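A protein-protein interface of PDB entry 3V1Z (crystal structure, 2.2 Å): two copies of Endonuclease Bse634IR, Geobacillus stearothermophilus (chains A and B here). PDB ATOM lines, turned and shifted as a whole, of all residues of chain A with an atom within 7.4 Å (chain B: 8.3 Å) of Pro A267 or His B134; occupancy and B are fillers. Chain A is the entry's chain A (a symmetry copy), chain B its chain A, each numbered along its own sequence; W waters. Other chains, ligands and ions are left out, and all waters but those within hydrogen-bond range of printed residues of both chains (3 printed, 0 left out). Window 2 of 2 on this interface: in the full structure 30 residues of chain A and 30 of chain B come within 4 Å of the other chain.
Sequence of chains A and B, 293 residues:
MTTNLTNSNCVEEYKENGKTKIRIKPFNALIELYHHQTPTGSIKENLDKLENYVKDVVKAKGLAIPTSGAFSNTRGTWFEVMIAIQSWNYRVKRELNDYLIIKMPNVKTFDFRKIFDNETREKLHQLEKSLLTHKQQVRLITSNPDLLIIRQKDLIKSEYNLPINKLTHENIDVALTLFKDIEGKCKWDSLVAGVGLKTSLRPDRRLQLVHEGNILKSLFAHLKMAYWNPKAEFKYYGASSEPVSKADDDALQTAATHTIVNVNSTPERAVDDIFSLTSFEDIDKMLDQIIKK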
ATOM      1  N   ALA A 255     -12.131  15.763 -26.038  1.00  0.00           N
ATOM      2  CA  ALA A 255     -12.750  16.894 -25.364  1.00  0.00           C
ATOM      3  C   ALA A 255     -14.228  17.006 -25.665  1.00  0.00           C
ATOM      4  O   ALA A 255     -14.686  16.621 -26.741  1.00  0.00           O
ATOM      5  CB  ALA A 255     -12.049  18.184 -25.766  1.00  0.00           C
ATOM      6  N   ALA A 256     -14.971  17.527 -24.691  1.00  0.00           N
ATOM      7  CA  ALA A 256     -16.285  18.095 -24.946  1.00  0.00           C
ATOM      8  C   ALA A 256     -15.997  19.398 -25.696  1.00  0.00           C
ATOM      9  O   ALA A 256     -15.482  20.354 -25.114  1.00  0.00           O
ATOM     10  CB  ALA A 256     -17.011  18.364 -23.630  1.00  0.00           C
ATOM     11  N   THR A 259     -15.909  23.306 -24.884  1.00  0.00           N
ATOM     12  CA  THR A 259     -15.018  23.794 -23.839  1.00  0.00           C
ATOM     13  C   THR A 259     -13.634  24.179 -24.368  1.00  0.00           C
ATOM     14  O   THR A 259     -12.808  24.680 -23.613  1.00  0.00           O
ATOM     15  CB  THR A 259     -14.849  22.753 -22.703  1.00  0.00           C
ATOM     16  OG1 THR A 259     -14.139  21.609 -23.196  1.00  0.00           O
ATOM     17  CG2 THR A 259     -16.203  22.319 -22.145  1.00  0.00           C
ATOM     18  N   ILE A 260     -13.383  23.956 -25.657  1.00  0.00           N
ATOM     19  CA  ILE A 260     -12.044  24.206 -26.224  1.00  0.00           C
ATOM     20  C   ILE A 260     -11.952  25.356 -27.245  1.00  0.00           C
ATOM     21  O   ILE A 260     -10.901  25.555 -27.857  1.00  0.00           O
ATOM     22  CB  ILE A 260     -11.418  22.912 -26.826  1.00  0.00           C
ATOM     23  CG1 ILE A 260     -12.227  22.420 -28.034  1.00  0.00           C
ATOM     24  CG2 ILE A 260     -11.317  21.823 -25.756  1.00  0.00           C
ATOM     25  CD1 ILE A 260     -11.412  21.653 -29.055  1.00  0.00           C
ATOM     26  N   ASN A 262     -11.855  28.679 -26.941  1.00  0.00           N
ATOM     27  CA  ASN A 262     -11.015  29.824 -26.610  1.00  0.00           C
ATOM     28  C   ASN A 262      -9.661  29.426 -26.013  1.00  0.00           C
ATOM     29  O   ASN A 262      -9.543  28.380 -25.378  1.00  0.00           O
ATOM     30  CB  ASN A 262     -11.785  30.769 -25.687  1.00  0.00           C
ATOM     31  CG  ASN A 262     -13.183  31.102 -26.220  1.00  0.00           C
ATOM     32  OD1 ASN A 262     -13.332  31.728 -27.280  1.00  0.00           O
ATOM     33  ND2 ASN A 262     -14.212  30.677 -25.487  1.00  0.00           N
ATOM     34  N   VAL A 263      -8.643  30.257 -26.231  1.00  0.00           N
ATOM     35  CA  VAL A 263      -7.265  29.939 -25.814  1.00  0.00           C
ATOM     36  C   VAL A 263      -7.084  29.815 -24.287  1.00  0.00           C
ATOM     37  O   VAL A 263      -6.203  29.086 -23.820  1.00  0.00           O
ATOM     38  CB  VAL A 263      -6.229  30.944 -26.422  1.00  0.00           C
ATOM     39  CG1 VAL A 263      -6.364  32.336 -25.800  1.00  0.00           C
ATOM     40  CG2 VAL A 263      -4.797  30.419 -26.289  1.00  0.00           C
ATOM     41  N   ASN A 264      -7.920  30.522 -23.525  1.00  0.00           N
ATOM     42  CA  ASN A 264      -7.828  30.529 -22.058  1.00  0.00           C
ATOM     43  C   ASN A 264      -8.980  29.794 -21.357  1.00  0.00           C
ATOM     44  O   ASN A 264      -9.224  29.992 -20.160  1.00  0.00           O
ATOM     45  CB  ASN A 264      -7.674  31.965 -21.527  1.00  0.00           C
ATOM     46  CG  ASN A 264      -6.290  32.543 -21.791  1.00  0.00           C
ATOM     47  OD1 ASN A 264      -6.132  33.428 -22.626  1.00  0.00           O
ATOM     48  ND2 ASN A 264      -5.281  32.036 -21.082  1.00  0.00           N
ATOM     49  N   SER A 265      -9.687  28.952 -22.116  1.00  0.00           N
ATOM     50  CA  SER A 265     -10.628  27.990 -21.547  1.00  0.00           C
ATOM     51  C   SER A 265      -9.836  26.834 -20.946  1.00  0.00           C
ATOM     52  O   SER A 265      -8.774  26.478 -21.458  1.00  0.00           O
ATOM     53  CB  SER A 265     -11.562  27.449 -22.633  1.00  0.00           C
ATOM     54  OG  SER A 265     -12.564  28.388 -22.996  1.00  0.00           O
ATOM     55  N   THR A 266     -10.329  26.268 -19.848  1.00  0.00           N
ATOM     56  CA  THR A 266      -9.790  25.000 -19.356  1.00  0.00           C
ATOM     57  C   THR A 266     -10.630  23.879 -19.973  1.00  0.00           C
ATOM     58  O   THR A 266     -11.837  23.776 -19.710  1.00  0.00           O
ATOM     59  CB  THR A 266      -9.741  24.907 -17.805  1.00  0.00           C
ATOM     60  OG1 THR A 266      -8.995  26.011 -17.280  1.00  0.00           O
ATOM     61  CG2 THR A 266      -9.059  23.615 -17.356  1.00  0.00           C
ATOM     62  N   PRO A 267      -9.998  23.053 -20.824  1.00  0.00           N
ATOM     63  CA  PRO A 267     -10.719  22.031 -21.563  1.00  0.00           C
ATOM     64  C   PRO A 267     -11.213  20.912 -20.644  1.00  0.00           C
ATOM     65  O   PRO A 267     -10.504  20.496 -19.725  1.00  0.00           O
ATOM     66  CB  PRO A 267      -9.665  21.492 -22.536  1.00  0.00           C
ATOM     67  CG  PRO A 267      -8.532  22.467 -22.493  1.00  0.00           C
ATOM     68  CD  PRO A 267      -8.560  23.025 -21.126  1.00  0.00           C
ATOM     69  N   GLU A 268     -12.433  20.455 -20.898  1.00  0.00           N
ATOM     70  CA  GLU A 268     -13.014  19.327 -20.192  1.00  0.00           C
ATOM     71  C   GLU A 268     -13.088  18.120 -21.124  1.00  0.00           C
ATOM     72  O   GLU A 268     -13.483  18.243 -22.295  1.00  0.00           O
ATOM     73  CB  GLU A 268     -14.415  19.688 -19.686  1.00  0.00           C
ATOM     74  CG  GLU A 268     -15.123  18.578 -18.928  1.00  0.00           C
ATOM     75  CD  GLU A 268     -16.469  18.997 -18.354  1.00  0.00           C
ATOM     76  OE1 GLU A 268     -17.064  19.973 -18.871  1.00  0.00           O
ATOM     77  OE2 GLU A 268     -16.927  18.342 -17.383  1.00  0.00           O
ATOM     78  N   ARG A 269     -12.691  16.961 -20.605  1.00  0.00           N
ATOM     79  CA  ARG A 269     -12.948  15.687 -21.268  1.00  0.00           C
ATOM     80  C   ARG A 269     -14.454  15.452 -21.327  1.00  0.00           C
ATOM     81  O   ARG A 269     -15.159  15.737 -20.360  1.00  0.00           O
ATOM     82  CB  ARG A 269     -12.290  14.545 -20.490  1.00  0.00           C
ATOM     83  CG  ARG A 269     -10.786  14.497 -20.623  1.00  0.00           C
ATOM     84  CD  ARG A 269     -10.179  13.441 -19.723  1.00  0.00           C
ATOM     85  NE  ARG A 269     -10.660  12.094 -20.037  1.00  0.00           N
ATOM     86  CZ  ARG A 269     -10.133  10.972 -19.548  1.00  0.00           C
ATOM     87  NH1 ARG A 269      -9.089  11.028 -18.720  1.00  0.00           N
ATOM     88  NH2 ARG A 269     -10.650   9.794 -19.893  1.00  0.00           N
ATOM     89  N   ALA A 270     -14.943  14.942 -22.457  1.00  0.00           N
ATOM     90  CA  ALA A 270     -16.349  14.517 -22.570  1.00  0.00           C
ATOM     91  C   ALA A 270     -16.623  13.311 -21.651  1.00  0.00           C
ATOM     92  O   ALA A 270     -17.689  13.209 -21.034  1.00  0.00           O
ATOM     93  CB  ALA A 270     -16.696  14.184 -24.015  1.00  0.00           C
ATOM     94  N   LEU B 127      -2.597  23.318 -31.317  1.00  0.00           N
ATOM     95  CA  LEU B 127      -3.849  23.009 -30.639  1.00  0.00           C
ATOM     96  C   LEU B 127      -3.736  21.718 -29.827  1.00  0.00           C
ATOM     97  O   LEU B 127      -4.096  21.698 -28.649  1.00  0.00           O
ATOM     98  CB  LEU B 127      -5.010  22.929 -31.637  1.00  0.00           C
ATOM     99  CG  LEU B 127      -6.355  22.392 -31.126  1.00  0.00           C
ATOM    100  CD1 LEU B 127      -6.974  23.302 -30.069  1.00  0.00           C
ATOM    101  CD2 LEU B 127      -7.308  22.173 -32.284  1.00  0.00           C
ATOM    102  N   GLU B 128      -3.230  20.660 -30.463  1.00  0.00           N
ATOM    103  CA  GLU B 128      -3.063  19.348 -29.834  1.00  0.00           C
ATOM    104  C   GLU B 128      -2.182  19.431 -28.595  1.00  0.00           C
ATOM    105  O   GLU B 128      -2.539  18.898 -27.540  1.00  0.00           O
ATOM    106  CB  GLU B 128      -2.477  18.334 -30.831  1.00  0.00           C
ATOM    107  CG  GLU B 128      -1.790  17.114 -30.186  1.00  0.00           C
ATOM    108  CD  GLU B 128      -1.333  16.073 -31.194  1.00  0.00           C
ATOM    109  OE1 GLU B 128      -0.858  16.445 -32.292  1.00  0.00           O
ATOM    110  OE2 GLU B 128      -1.442  14.871 -30.880  1.00  0.00           O
ATOM    111  N   LYS B 129      -1.046  20.115 -28.737  1.00  0.00           N
ATOM    112  CA  LYS B 129      -0.056  20.234 -27.677  1.00  0.00           C
ATOM    113  C   LYS B 129      -0.544  21.096 -26.519  1.00  0.00           C
ATOM    114  O   LYS B 129      -0.231  20.806 -25.365  1.00  0.00           O
ATOM    115  CB  LYS B 129       1.272  20.767 -28.227  1.00  0.00           C
ATOM    116  CG  LYS B 129       2.484  20.424 -27.363  1.00  0.00           C
ATOM    117  CD  LYS B 129       3.750  20.249 -28.208  1.00  0.00           C
ATOM    118  CE  LYS B 129       4.866  19.576 -27.408  1.00  0.00           C
ATOM    119  NZ  LYS B 129       5.943  19.021 -28.290  1.00  0.00           N
ATOM    120  N   SER B 130      -1.312  22.144 -26.825  1.00  0.00           N
ATOM    121  CA  SER B 130      -1.880  23.004 -25.779  1.00  0.00           C
ATOM    122  C   SER B 130      -2.987  22.282 -25.009  1.00  0.00           C
ATOM    123  O   SER B 130      -3.113  22.446 -23.797  1.00  0.00           O
ATOM    124  CB  SER B 130      -2.388  24.331 -26.347  1.00  0.00           C
ATOM    125  OG  SER B 130      -3.719  24.216 -26.824  1.00  0.00           O
ATOM    126  N   LEU B 131      -3.777  21.477 -25.718  1.00  0.00           N
ATOM    127  CA  LEU B 131      -4.842  20.686 -25.092  1.00  0.00           C
ATOM    128  C   LEU B 131      -4.306  19.685 -24.062  1.00  0.00           C
ATOM    129  O   LEU B 131      -4.990  19.366 -23.086  1.00  0.00           O
ATOM    130  CB  LEU B 131      -5.710  19.986 -26.153  1.00  0.00           C
ATOM    131  CG  LEU B 131      -6.716  20.838 -26.950  1.00  0.00           C
ATOM    132  CD1 LEU B 131      -7.403  20.011 -28.022  1.00  0.00           C
ATOM    133  CD2 LEU B 131      -7.756  21.509 -26.063  1.00  0.00           C
ATOM    134  N   LEU B 132      -3.079  19.211 -24.288  1.00  0.00           N
ATOM    135  CA  LEU B 132      -2.371  18.336 -23.350  1.00  0.00           C
ATOM    136  C   LEU B 132      -1.643  19.101 -22.234  1.00  0.00           C
ATOM    137  O   LEU B 132      -1.164  18.488 -21.272  1.00  0.00           O
ATOM    138  CB  LEU B 132      -1.352  17.463 -24.092  1.00  0.00           C
ATOM    139  CG  LEU B 132      -1.737  16.472 -25.191  1.00  0.00           C
ATOM    140  CD1 LEU B 132      -0.466  15.855 -25.756  1.00  0.00           C
ATOM    141  CD2 LEU B 132      -2.681  15.389 -24.689  1.00  0.00           C
ATOM    142  N   THR B 133      -1.534  20.424 -22.369  1.00  0.00           N
ATOM    143  CA  THR B 133      -0.822  21.245 -21.378  1.00  0.00           C
ATOM    144  C   THR B 133      -1.777  21.698 -20.275  1.00  0.00           C
ATOM    145  O   THR B 133      -1.943  22.898 -20.019  1.00  0.00           O
ATOM    146  CB  THR B 133      -0.133  22.490 -22.002  1.00  0.00           C
ATOM    147  OG1 THR B 133       0.373  22.177 -23.304  1.00  0.00           O
ATOM    148  CG2 THR B 133       1.015  22.965 -21.116  1.00  0.00           C
ATOM    149  N   HIS B 134      -2.415  20.726 -19.637  1.00  0.00           N
ATOM    150  CA  HIS B 134      -3.318  20.985 -18.527  1.00  0.00           C
ATOM    151  C   HIS B 134      -3.207  19.841 -17.537  1.00  0.00           C
ATOM    152  O   HIS B 134      -2.616  18.800 -17.844  1.00  0.00           O
ATOM    153  CB  HIS B 134      -4.765  21.138 -19.015  1.00  0.00           C
ATOM    154  CG  HIS B 134      -4.978  22.307 -19.928  1.00  0.00           C
ATOM    155  ND1 HIS B 134      -5.119  22.171 -21.293  1.00  0.00           N
ATOM    156  CD2 HIS B 134      -5.071  23.634 -19.669  1.00  0.00           C
ATOM    157  CE1 HIS B 134      -5.286  23.365 -21.837  1.00  0.00           C
ATOM    158  NE2 HIS B 134      -5.262  24.269 -20.873  1.00  0.00           N
ATOM    159  N   LYS B 135      -3.751  20.052 -16.341  1.00  0.00           N
ATOM    160  CA  LYS B 135      -3.838  19.010 -15.321  1.00  0.00           C
ATOM    161  C   LYS B 135      -4.583  17.803 -15.889  1.00  0.00           C
ATOM    162  O   LYS B 135      -4.064  16.684 -15.881  1.00  0.00           O
ATOM    163  CB  LYS B 135      -4.515  19.549 -14.049  1.00  0.00           C
ATOM    164  CG  LYS B 135      -5.618  20.585 -14.310  1.00  0.00           C
ATOM    165  CD  LYS B 135      -6.097  21.263 -13.029  1.00  0.00           C
ATOM    166  CE  LYS B 135      -7.384  22.057 -13.278  1.00  0.00           C
ATOM    167  NZ  LYS B 135      -7.832  22.815 -12.069  1.00  0.00           N
ATOM    168  N   GLN B 136      -5.789  18.044 -16.402  1.00  0.00           N
ATOM    169  CA  GLN B 136      -6.548  17.026 -17.110  1.00  0.00           C
ATOM    170  C   GLN B 136      -6.255  17.159 -18.602  1.00  0.00           C
ATOM    171  O   GLN B 136      -6.672  18.129 -19.240  1.00  0.00           O
ATOM    172  CB  GLN B 136      -8.053  17.163 -16.826  1.00  0.00           C
ATOM    173  CG  GLN B 136      -8.907  16.069 -17.468  1.00  0.00           C
ATOM    174  CD  GLN B 136     -10.351  16.076 -16.983  1.00  0.00           C
ATOM    175  OE1 GLN B 136     -10.702  15.357 -16.043  1.00  0.00           O
ATOM    176  NE2 GLN B 136     -11.193  16.880 -17.626  1.00  0.00           N
ATOM    177  N   GLN B 137      -5.522  16.188 -19.141  1.00  0.00           N
ATOM    178  CA  GLN B 137      -5.138  16.185 -20.551  1.00  0.00           C
ATOM    179  C   GLN B 137      -6.323  15.808 -21.438  1.00  0.00           C
ATOM    180  O   GLN B 137      -7.025  14.833 -21.163  1.00  0.00           O
ATOM    181  CB  GLN B 137      -3.962  15.228 -20.791  1.00  0.00           C
ATOM    182  CG  GLN B 137      -2.745  15.537 -19.919  1.00  0.00           C
ATOM    183  CD  GLN B 137      -1.455  14.890 -20.406  1.00  0.00           C
ATOM    184  OE1 GLN B 137      -1.468  13.891 -21.131  1.00  0.00           O
ATOM    185  NE2 GLN B 137      -0.328  15.459 -19.993  1.00  0.00           N
ATOM    186  N   VAL B 138      -6.555  16.603 -22.481  1.00  0.00           N
ATOM    187  CA  VAL B 138      -7.610  16.297 -23.453  1.00  0.00           C
ATOM    188  C   VAL B 138      -7.069  16.169 -24.878  1.00  0.00           C
ATOM    189  O   VAL B 138      -5.966  16.637 -25.190  1.00  0.00           O
ATOM    190  CB  VAL B 138      -8.840  17.271 -23.381  1.00  0.00           C
ATOM    191  CG1 VAL B 138      -9.271  17.519 -21.940  1.00  0.00           C
ATOM    192  CG2 VAL B 138      -8.555  18.570 -24.077  1.00  0.00           C
ATOM    193  N   ARG B 139      -7.840  15.495 -25.723  1.00  0.00           N
ATOM    194  CA  ARG B 139      -7.474  15.255 -27.109  1.00  0.00           C
ATOM    195  C   ARG B 139      -8.674  15.512 -28.004  1.00  0.00           C
ATOM    196  O   ARG B 139      -9.754  15.846 -27.519  1.00  0.00           O
ATOM    197  CB  ARG B 139      -6.991  13.814 -27.291  1.00  0.00           C
ATOM    198  CG  ARG B 139      -5.708  13.488 -26.544  1.00  0.00           C
ATOM    199  CD  ARG B 139      -5.341  12.029 -26.682  1.00  0.00           C
ATOM    200  NE  ARG B 139      -4.391  11.629 -25.643  1.00  0.00           N
ATOM    201  CZ  ARG B 139      -3.069  11.633 -25.774  1.00  0.00           C
ATOM    202  NH1 ARG B 139      -2.506  12.015 -26.914  1.00  0.00           N
ATOM    203  NH2 ARG B 139      -2.306  11.253 -24.759  1.00  0.00           N
HETATM  204  O   HOH W   1     -11.723  20.008 -16.833  1.00  0.00           O
HETATM  205  O   HOH W   2      -7.141  12.954 -18.999  1.00  0.00           O
HETATM  206  O   HOH W   3      -8.157  20.324 -18.892  1.00  0.00           O
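O of Arg B139 is in hydrogen-bond range of N of Ala A255.
The side-chain amide nitrogen (NE2) of Gln B136 sits close to the backbone NH (N) of Arg A269 (3.3 Å).
The backbone carbonyl oxygen (O) of Glu A268 sits at hydrogen-bond distance from the backbone NH (N) of Ala A256.
O of Ser B130 lies close to ND1 of His B134 (3.2 Å).
The backbone carbonyl oxygen (O) of Leu B131 is in hydrogen-bond range of the backbone NH (N) of Val B138, at 3.2 Å.
The backbone carbonyl oxygen (O) of Leu B131 lies within hydrogen-bond range of a ring nitrogen (ND1) of His B134 (3.3 Å).
The backbone carbonyl oxygen (O) of Leu B132 is in hydrogen-bond range of the side-chain amide nitrogen (NE2) of Gln B137 (3.4 Å).
OG1 of Thr A259 sits at hydrogen-bond distance from N of Glu A268.
Val B138 touches Ala A255 (CG2 to CB, 3.9 Å).
CD2 of Leu B131 touches CG2 of Ile A260 (3.6 Å).
Pro A267 touches Leu B131.
His B134 touches Pro A267.
CG2 of Val B138 touches CB of Pro A267 (3.5 Å).
CA of Glu A268 touches NE2 of Gln B136 (3.99 Å).
Val B138 touches Glu A268.
Gln B137 touches Arg A269 (O to CD, 3.7 Å).
CG1 of Val B138 touches CG of Arg A269, 3.6 Å away.
Ala A256 touches none of the printed residues of chain B.
Asn A262 touches none of the printed residues of chain B.
Pro A267 touches three residues of chain B.
Printed residues of chain B within 4 Å of Arg A269: Gln B136 (3.3 Å), Gln B137 (3.7 Å) and Val B138 (3.6 Å).
Of the printed residues of chain A, Leu B131 touches Ile A260 and Pro A267.
His B134 touches one residue of chain A.
Of the printed residues of chain A, Gln B137 touches Arg A269 (3.7 Å).
The nearest residue of chain B that does not touch Pro A267 is Gln B136 (4.2 Å).
The nearest residue of chain A that does not touch His B134 is Ser A265 (4.2 Å).
Of the 13 printed residues of chain B, 6 touch a printed residue of chain A.
Among the printed residues, no Asp or Glu carboxylate lies within 4 Å of a Lys or Arg side-chain nitrogen of the other chain.
No position is printed for both chains.
Water W3 lies within hydrogen-bond range of the backbone carbonyl oxygen of Pro A267 and the backbone carbonyl oxygen of Gln B136.
Water W2 lies within hydrogen-bond range of NH1 of Arg A269 (2.8 Å) and O of Gln B137 (2.9 Å).
Water W1 lies within hydrogen-bond range of O of Pro A267 (3.2 Å) and NE2 of Gln B136 (3.3 Å).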
